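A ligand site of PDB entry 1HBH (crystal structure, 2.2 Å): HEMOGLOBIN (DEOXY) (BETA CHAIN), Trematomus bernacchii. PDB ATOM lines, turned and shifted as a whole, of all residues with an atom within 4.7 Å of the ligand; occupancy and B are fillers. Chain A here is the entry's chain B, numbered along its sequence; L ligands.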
ATOM      1  N   THR A  38      -5.453  20.482 -25.182  1.00  0.00           N
ATOM      2  CA  THR A  38      -4.453  19.906 -24.221  1.00  0.00           C
ATOM      3  C   THR A  38      -5.081  18.873 -23.318  1.00  0.00           C
ATOM      4  O   THR A  38      -4.365  18.155 -22.571  1.00  0.00           O
ATOM      5  CB  THR A  38      -3.657  20.998 -23.427  1.00  0.00           C
ATOM      6  OG1 THR A  38      -4.624  21.681 -22.559  1.00  0.00           O
ATOM      7  CG2 THR A  38      -2.963  22.038 -24.351  1.00  0.00           C
ATOM      8  N   HIS A  41      -4.206  14.358 -23.473  1.00  0.00           N
ATOM      9  CA  HIS A  41      -3.360  13.515 -22.662  1.00  0.00           C
ATOM     10  C   HIS A  41      -3.835  13.261 -21.243  1.00  0.00           C
ATOM     11  O   HIS A  41      -2.948  12.971 -20.403  1.00  0.00           O
ATOM     12  CB  HIS A  41      -1.954  14.250 -22.542  1.00  0.00           C
ATOM     13  CG  HIS A  41      -1.469  14.479 -23.965  1.00  0.00           C
ATOM     14  ND1 HIS A  41      -0.900  13.497 -24.755  1.00  0.00           N
ATOM     15  CD2 HIS A  41      -1.569  15.599 -24.720  1.00  0.00           C
ATOM     16  CE1 HIS A  41      -0.656  14.024 -25.936  1.00  0.00           C
ATOM     17  NE2 HIS A  41      -1.044  15.278 -25.959  1.00  0.00           N
ATOM     18  N   PHE A  42      -5.098  13.412 -20.926  1.00  0.00           N
ATOM     19  CA  PHE A  42      -5.588  13.320 -19.556  1.00  0.00           C
ATOM     20  C   PHE A  42      -6.829  12.464 -19.370  1.00  0.00           C
ATOM     21  O   PHE A  42      -7.584  12.745 -18.419  1.00  0.00           O
ATOM     22  CB  PHE A  42      -5.712  14.753 -18.969  1.00  0.00           C
ATOM     23  CG  PHE A  42      -4.393  15.474 -18.898  1.00  0.00           C
ATOM     24  CD1 PHE A  42      -3.411  15.112 -17.967  1.00  0.00           C
ATOM     25  CD2 PHE A  42      -4.120  16.488 -19.828  1.00  0.00           C
ATOM     26  CE1 PHE A  42      -2.181  15.765 -17.948  1.00  0.00           C
ATOM     27  CE2 PHE A  42      -2.906  17.166 -19.813  1.00  0.00           C
ATOM     28  CZ  PHE A  42      -1.931  16.804 -18.853  1.00  0.00           C
ATOM     29  N   HIS A  63      -0.946  16.977 -10.924  1.00  0.00           N
ATOM     30  CA  HIS A  63      -0.012  16.978 -12.094  1.00  0.00           C
ATOM     31  C   HIS A  63       0.486  18.416 -12.360  1.00  0.00           C
ATOM     32  O   HIS A  63       1.485  18.709 -13.046  1.00  0.00           O
ATOM     33  CB  HIS A  63      -0.637  16.384 -13.350  1.00  0.00           C
ATOM     34  CG  HIS A  63       0.271  16.219 -14.516  1.00  0.00           C
ATOM     35  ND1 HIS A  63       1.238  15.235 -14.604  1.00  0.00           N
ATOM     36  CD2 HIS A  63       0.362  16.932 -15.658  1.00  0.00           C
ATOM     37  CE1 HIS A  63       1.867  15.353 -15.744  1.00  0.00           C
ATOM     38  NE2 HIS A  63       1.379  16.393 -16.410  1.00  0.00           N
ATOM     39  N   LYS A  66       3.422  18.761 -10.255  1.00  0.00           N
ATOM     40  CA  LYS A  66       4.472  17.948 -10.883  1.00  0.00           C
ATOM     41  C   LYS A  66       5.204  18.783 -11.936  1.00  0.00           C
ATOM     42  O   LYS A  66       6.432  19.042 -11.861  1.00  0.00           O
ATOM     43  CB  LYS A  66       3.957  16.681 -11.573  1.00  0.00           C
ATOM     44  CG  LYS A  66       4.690  15.430 -11.212  1.00  0.00           C
ATOM     45  CD  LYS A  66       4.221  14.132 -11.760  1.00  0.00           C
ATOM     46  CE  LYS A  66       2.912  13.602 -11.234  1.00  0.00           C
ATOM     47  NZ  LYS A  66       2.045  13.043 -12.357  1.00  0.00           N
ATOM     48  N   VAL A  67       4.436  19.205 -12.935  1.00  0.00           N
ATOM     49  CA  VAL A  67       4.996  19.993 -14.048  1.00  0.00           C
ATOM     50  C   VAL A  67       5.685  21.264 -13.595  1.00  0.00           C
ATOM     51  O   VAL A  67       6.772  21.533 -14.179  1.00  0.00           O
ATOM     52  CB  VAL A  67       3.868  20.187 -15.088  1.00  0.00           C
ATOM     53  CG1 VAL A  67       4.258  21.185 -16.167  1.00  0.00           C
ATOM     54  CG2 VAL A  67       3.433  18.851 -15.654  1.00  0.00           C
ATOM     55  N   GLY A  70       9.119  20.711 -12.318  1.00  0.00           N
ATOM     56  CA  GLY A  70       9.767  20.347 -13.549  1.00  0.00           C
ATOM     57  C   GLY A  70      10.708  21.452 -14.029  1.00  0.00           C
ATOM     58  O   GLY A  70      11.684  21.133 -14.772  1.00  0.00           O
ATOM     59  N   LEU A  71      10.478  22.685 -13.647  1.00  0.00           N
ATOM     60  CA  LEU A  71      11.392  23.804 -14.038  1.00  0.00           C
ATOM     61  C   LEU A  71      12.505  23.982 -13.003  1.00  0.00           C
ATOM     62  O   LEU A  71      13.471  24.762 -13.188  1.00  0.00           O
ATOM     63  CB  LEU A  71      10.522  25.057 -14.210  1.00  0.00           C
ATOM     64  CG  LEU A  71       9.185  25.003 -14.919  1.00  0.00           C
ATOM     65  CD1 LEU A  71       8.423  26.279 -14.828  1.00  0.00           C
ATOM     66  CD2 LEU A  71       9.424  24.651 -16.399  1.00  0.00           C
ATOM     67  N   ARG A  73      14.930  22.064 -12.072  1.00  0.00           N
ATOM     68  CA  ARG A  73      16.205  21.630 -12.647  1.00  0.00           C
ATOM     69  C   ARG A  73      16.741  22.676 -13.587  1.00  0.00           C
ATOM     70  O   ARG A  73      17.977  22.904 -13.598  1.00  0.00           O
ATOM     71  CB  ARG A  73      16.122  20.263 -13.274  1.00  0.00           C
ATOM     72  CG  ARG A  73      15.470  20.157 -14.628  1.00  0.00           C
ATOM     73  CD  ARG A  73      15.386  18.662 -14.946  1.00  0.00           C
ATOM     74  NE  ARG A  73      14.377  18.045 -14.064  1.00  0.00           N
ATOM     75  CZ  ARG A  73      13.862  16.843 -14.388  1.00  0.00           C
ATOM     76  NH1 ARG A  73      14.277  16.152 -15.454  1.00  0.00           N
ATOM     77  NH2 ARG A  73      12.917  16.336 -13.612  1.00  0.00           N
ATOM     78  N   LEU A  88      13.572  14.467 -20.600  1.00  0.00           N
ATOM     79  CA  LEU A  88      12.125  14.834 -20.446  1.00  0.00           C
ATOM     80  C   LEU A  88      11.537  15.032 -21.848  1.00  0.00           C
ATOM     81  O   LEU A  88      10.348  14.723 -22.111  1.00  0.00           O
ATOM     82  CB  LEU A  88      12.066  16.006 -19.502  1.00  0.00           C
ATOM     83  CG  LEU A  88      10.860  16.297 -18.638  1.00  0.00           C
ATOM     84  CD1 LEU A  88      10.458  15.126 -17.734  1.00  0.00           C
ATOM     85  CD2 LEU A  88      11.171  17.499 -17.753  1.00  0.00           C
ATOM     86  N   LEU A  91      11.002  11.611 -23.256  1.00  0.00           N
ATOM     87  CA  LEU A  91       9.766  11.125 -22.665  1.00  0.00           C
ATOM     88  C   LEU A  91       8.492  11.649 -23.350  1.00  0.00           C
ATOM     89  O   LEU A  91       7.555  10.896 -23.660  1.00  0.00           O
ATOM     90  CB  LEU A  91       9.841  11.490 -21.178  1.00  0.00           C
ATOM     91  CG  LEU A  91       8.576  11.018 -20.436  1.00  0.00           C
ATOM     92  CD1 LEU A  91       8.629   9.487 -20.416  1.00  0.00           C
ATOM     93  CD2 LEU A  91       8.548  11.689 -19.068  1.00  0.00           C
ATOM     94  N   HIS A  92       8.405  12.981 -23.477  1.00  0.00           N
ATOM     95  CA  HIS A  92       7.213  13.631 -24.040  1.00  0.00           C
ATOM     96  C   HIS A  92       6.989  13.325 -25.508  1.00  0.00           C
ATOM     97  O   HIS A  92       5.812  13.229 -25.941  1.00  0.00           O
ATOM     98  CB  HIS A  92       7.185  15.144 -23.795  1.00  0.00           C
ATOM     99  CG  HIS A  92       6.922  15.482 -22.346  1.00  0.00           C
ATOM    100  ND1 HIS A  92       7.904  15.528 -21.362  1.00  0.00           N
ATOM    101  CD2 HIS A  92       5.782  15.859 -21.731  1.00  0.00           C
ATOM    102  CE1 HIS A  92       7.361  15.887 -20.224  1.00  0.00           C
ATOM    103  NE2 HIS A  92       6.086  16.103 -20.418  1.00  0.00           N
ATOM    104  N   LEU A  96       4.839   9.869 -24.364  1.00  0.00           N
ATOM    105  CA  LEU A  96       3.564  10.638 -24.198  1.00  0.00           C
ATOM    106  C   LEU A  96       3.039  11.145 -25.529  1.00  0.00           C
ATOM    107  O   LEU A  96       1.821  11.412 -25.585  1.00  0.00           O
ATOM    108  CB  LEU A  96       3.717  11.705 -23.092  1.00  0.00           C
ATOM    109  CG  LEU A  96       4.568  11.233 -21.876  1.00  0.00           C
ATOM    110  CD1 LEU A  96       4.887  12.319 -20.907  1.00  0.00           C
ATOM    111  CD2 LEU A  96       3.746  10.127 -21.197  1.00  0.00           C
ATOM    112  N   VAL A  98       3.216  13.991 -26.829  1.00  0.00           N
ATOM    113  CA  VAL A  98       2.665  15.320 -26.595  1.00  0.00           C
ATOM    114  C   VAL A  98       3.048  16.350 -27.649  1.00  0.00           C
ATOM    115  O   VAL A  98       4.243  16.668 -27.718  1.00  0.00           O
ATOM    116  CB  VAL A  98       3.144  15.754 -25.183  1.00  0.00           C
ATOM    117  CG1 VAL A  98       2.522  17.128 -24.872  1.00  0.00           C
ATOM    118  CG2 VAL A  98       2.806  14.780 -24.120  1.00  0.00           C
ATOM    119  N   ASN A 102       1.880  22.598 -27.236  1.00  0.00           N
ATOM    120  CA  ASN A 102       1.223  22.582 -25.909  1.00  0.00           C
ATOM    121  C   ASN A 102       2.181  23.105 -24.818  1.00  0.00           C
ATOM    122  O   ASN A 102       1.666  23.649 -23.822  1.00  0.00           O
ATOM    123  CB  ASN A 102       0.666  21.181 -25.645  1.00  0.00           C
ATOM    124  CG  ASN A 102      -0.514  20.865 -26.556  1.00  0.00           C
ATOM    125  OD1 ASN A 102      -1.018  19.730 -26.497  1.00  0.00           O
ATOM    126  ND2 ASN A 102      -0.988  21.805 -27.350  1.00  0.00           N
ATOM    127  N   PHE A 103       3.485  22.919 -24.975  1.00  0.00           N
ATOM    128  CA  PHE A 103       4.495  23.384 -23.983  1.00  0.00           C
ATOM    129  C   PHE A 103       4.388  24.933 -23.896  1.00  0.00           C
ATOM    130  O   PHE A 103       4.361  25.592 -22.831  1.00  0.00           O
ATOM    131  CB  PHE A 103       5.903  22.926 -24.318  1.00  0.00           C
ATOM    132  CG  PHE A 103       6.149  21.432 -24.385  1.00  0.00           C
ATOM    133  CD1 PHE A 103       5.559  20.553 -23.480  1.00  0.00           C
ATOM    134  CD2 PHE A 103       7.017  20.910 -25.378  1.00  0.00           C
ATOM    135  CE1 PHE A 103       5.809  19.157 -23.575  1.00  0.00           C
ATOM    136  CE2 PHE A 103       7.293  19.558 -25.485  1.00  0.00           C
ATOM    137  CZ  PHE A 103       6.668  18.688 -24.582  1.00  0.00           C
ATOM    138  N   LEU A 106       1.019  26.053 -22.171  1.00  0.00           N
ATOM    139  CA  LEU A 106       1.055  25.965 -20.705  1.00  0.00           C
ATOM    140  C   LEU A 106       1.902  27.087 -20.143  1.00  0.00           C
ATOM    141  O   LEU A 106       1.644  27.557 -19.019  1.00  0.00           O
ATOM    142  CB  LEU A 106       1.481  24.573 -20.240  1.00  0.00           C
ATOM    143  CG  LEU A 106       1.596  24.439 -18.712  1.00  0.00           C
ATOM    144  CD1 LEU A 106       0.225  24.613 -18.048  1.00  0.00           C
ATOM    145  CD2 LEU A 106       2.173  23.070 -18.412  1.00  0.00           C
ATOM    146  N   ILE A 110       1.168  29.699 -17.191  1.00  0.00           N
ATOM    147  CA  ILE A 110       2.018  29.868 -15.979  1.00  0.00           C
ATOM    148  C   ILE A 110       2.275  31.342 -15.774  1.00  0.00           C
ATOM    149  O   ILE A 110       2.158  31.914 -14.684  1.00  0.00           O
ATOM    150  CB  ILE A 110       3.324  29.020 -16.094  1.00  0.00           C
ATOM    151  CG1 ILE A 110       2.931  27.539 -16.267  1.00  0.00           C
ATOM    152  CG2 ILE A 110       4.309  29.226 -14.916  1.00  0.00           C
ATOM    153  CD1 ILE A 110       4.137  26.636 -16.671  1.00  0.00           C
ATOM    154  N   LEU A 141      12.539  21.314 -24.383  1.00  0.00           N
ATOM    155  CA  LEU A 141      11.573  20.194 -24.307  1.00  0.00           C
ATOM    156  C   LEU A 141      11.255  19.654 -25.704  1.00  0.00           C
ATOM    157  O   LEU A 141      10.910  18.466 -25.841  1.00  0.00           O
ATOM    158  CB  LEU A 141      10.364  20.694 -23.507  1.00  0.00           C
ATOM    159  CG  LEU A 141      10.345  20.587 -22.013  1.00  0.00           C
ATOM    160  CD1 LEU A 141       8.884  20.840 -21.519  1.00  0.00           C
ATOM    161  CD2 LEU A 141      10.764  19.154 -21.611  1.00  0.00           C
HETATM  162  C1  LIG L   1       5.012  14.142 -17.101  1.00  0.00           C
HETATM  163  C2  LIG L   1       7.237  18.447 -16.910  1.00  0.00           C
HETATM  164  C3  LIG L   1       4.179  20.242 -20.235  1.00  0.00           C
HETATM  165  C4  LIG L   1       1.802  15.976 -20.269  1.00  0.00           C
HETATM  166  C5  LIG L   1       5.927  15.129 -16.760  1.00  0.00           C
HETATM  167  C6  LIG L   1       7.106  15.025 -15.936  1.00  0.00           C
HETATM  168  C7  LIG L   1       7.677  16.247 -15.870  1.00  0.00           C
HETATM  169  C8  LIG L   1       6.866  17.143 -16.687  1.00  0.00           C
HETATM  170  C9  LIG L   1       8.975  16.668 -15.138  1.00  0.00           C
HETATM  171  C10 LIG L   1       7.706  13.831 -15.215  1.00  0.00           C
HETATM  172  C11 LIG L   1       6.964  12.578 -15.018  1.00  0.00           C
HETATM  173  C12 LIG L   1       7.855  11.360 -14.755  1.00  0.00           C
HETATM  174  O1  LIG L   1       9.092  11.594 -14.646  1.00  0.00           O
HETATM  175  O2  LIG L   1       7.148  10.323 -14.670  1.00  0.00           O
HETATM  176  C13 LIG L   1       6.651  19.233 -17.874  1.00  0.00           C
HETATM  177  C14 LIG L   1       7.032  20.604 -18.113  1.00  0.00           C
HETATM  178  C15 LIG L   1       6.163  21.097 -18.981  1.00  0.00           C
HETATM  179  C16 LIG L   1       5.227  20.026 -19.332  1.00  0.00           C
HETATM  180  C17 LIG L   1       8.224  21.285 -17.407  1.00  0.00           C
HETATM  181  C18 LIG L   1       6.105  22.491 -19.631  1.00  0.00           C
HETATM  182  C19 LIG L   1       6.659  23.560 -19.012  1.00  0.00           C
HETATM  183  C20 LIG L   1       3.278  19.227 -20.448  1.00  0.00           C
HETATM  184  C21 LIG L   1       2.100  19.392 -21.318  1.00  0.00           C
HETATM  185  C22 LIG L   1       1.479  18.215 -21.356  1.00  0.00           C
HETATM  186  C23 LIG L   1       2.183  17.274 -20.535  1.00  0.00           C
HETATM  187  C24 LIG L   1       1.805  20.726 -22.020  1.00  0.00           C
HETATM  188  C25 LIG L   1       0.201  17.871 -22.137  1.00  0.00           C
HETATM  189  C26 LIG L   1      -0.236  18.846 -22.961  1.00  0.00           C
HETATM  190  C27 LIG L   1       2.436  15.097 -19.385  1.00  0.00           C
HETATM  191  C28 LIG L   1       2.047  13.740 -19.106  1.00  0.00           C
HETATM  192  C29 LIG L   1       2.945  13.226 -18.279  1.00  0.00           C
HETATM  193  C30 LIG L   1       3.936  14.212 -17.977  1.00  0.00           C
HETATM  194  C31 LIG L   1       0.775  13.079 -19.689  1.00  0.00           C
HETATM  195  C32 LIG L   1       2.924  11.811 -17.596  1.00  0.00           C
HETATM  196  C33 LIG L   1       2.311  11.878 -16.178  1.00  0.00           C
HETATM  197  C34 LIG L   1       1.954  10.529 -15.582  1.00  0.00           C
HETATM  198  O3  LIG L   1       0.825  10.043 -15.837  1.00  0.00           O
HETATM  199  O4  LIG L   1       2.866  10.047 -14.842  1.00  0.00           O
HETATM  200  N1  LIG L   1       5.812  16.435 -17.227  1.00  0.00           N
HETATM  201  N2  LIG L   1       5.537  18.884 -18.630  1.00  0.00           N
HETATM  202  N3  LIG L   1       3.313  17.903 -19.973  1.00  0.00           N
HETATM  203  N4  LIG L   1       3.626  15.371 -18.693  1.00  0.00           N
HETATM  204 FE1  LIG L   1       4.746  16.989 -18.844  1.00  0.00          FE
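FE1 of the ligand is bound by NE2 of His 92, 2.2 Å away. An oxygen (O4) of the ligand lies within salt-bridge range of the side-chain amino group (NZ) of Lys 66, 3.98 Å away.
O of Leu 88 sits at hydrogen-bond distance from ND1 of His 92 (2.7 Å). The backbone carbonyl oxygen (O) of His 92 lies within hydrogen-bond range of the backbone NH (N) of Val 98, at 2.8 Å. O of Leu 91 sits at hydrogen-bond distance from N of Leu 96, 3.0 Å away. The side-chain amino group of Lys 66 is in hydrogen-bond range of a ring nitrogen (ND1) of His 63.
NE2 of His 63 lies close to N4 of the ligand, at 3.4 Å. His 41 touches the ligand. Phe 42 touches the ligand (CE2 to C25, 3.9 Å). Val 67 touches the ligand. CD2 of Leu 71 touches C17 of the ligand (3.7 Å). CD1 of Leu 88 touches C9 of the ligand, at 3.4 Å. CD1 of Leu 96 touches C29 of the ligand (3.4 Å). CG1 of Val 98 touches C25 of the ligand (3.7 Å). O of Asn 102 touches C24 of the ligand (3.4 Å). CD1 of Phe 103 touches C3 of the ligand (3.5 Å). CD2 of Leu 106 touches C3 of the ligand (3.9 Å). Leu 141 touches the ligand. Hydrophobic or aromatic side chains that line the ligand: His 41, Phe 42, His 63, Val 67, Leu 71, Leu 88, His 92, Leu 96, Val 98, Phe 103, Leu 106 and Leu 141. Within 4 Å of the ligand: His 41, Phe 42, His 63, Lys 66, Val 67, Leu 71, Leu 88, His 92, Leu 96, Val 98, Asn 102, Phe 103, Leu 106 and Leu 141.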
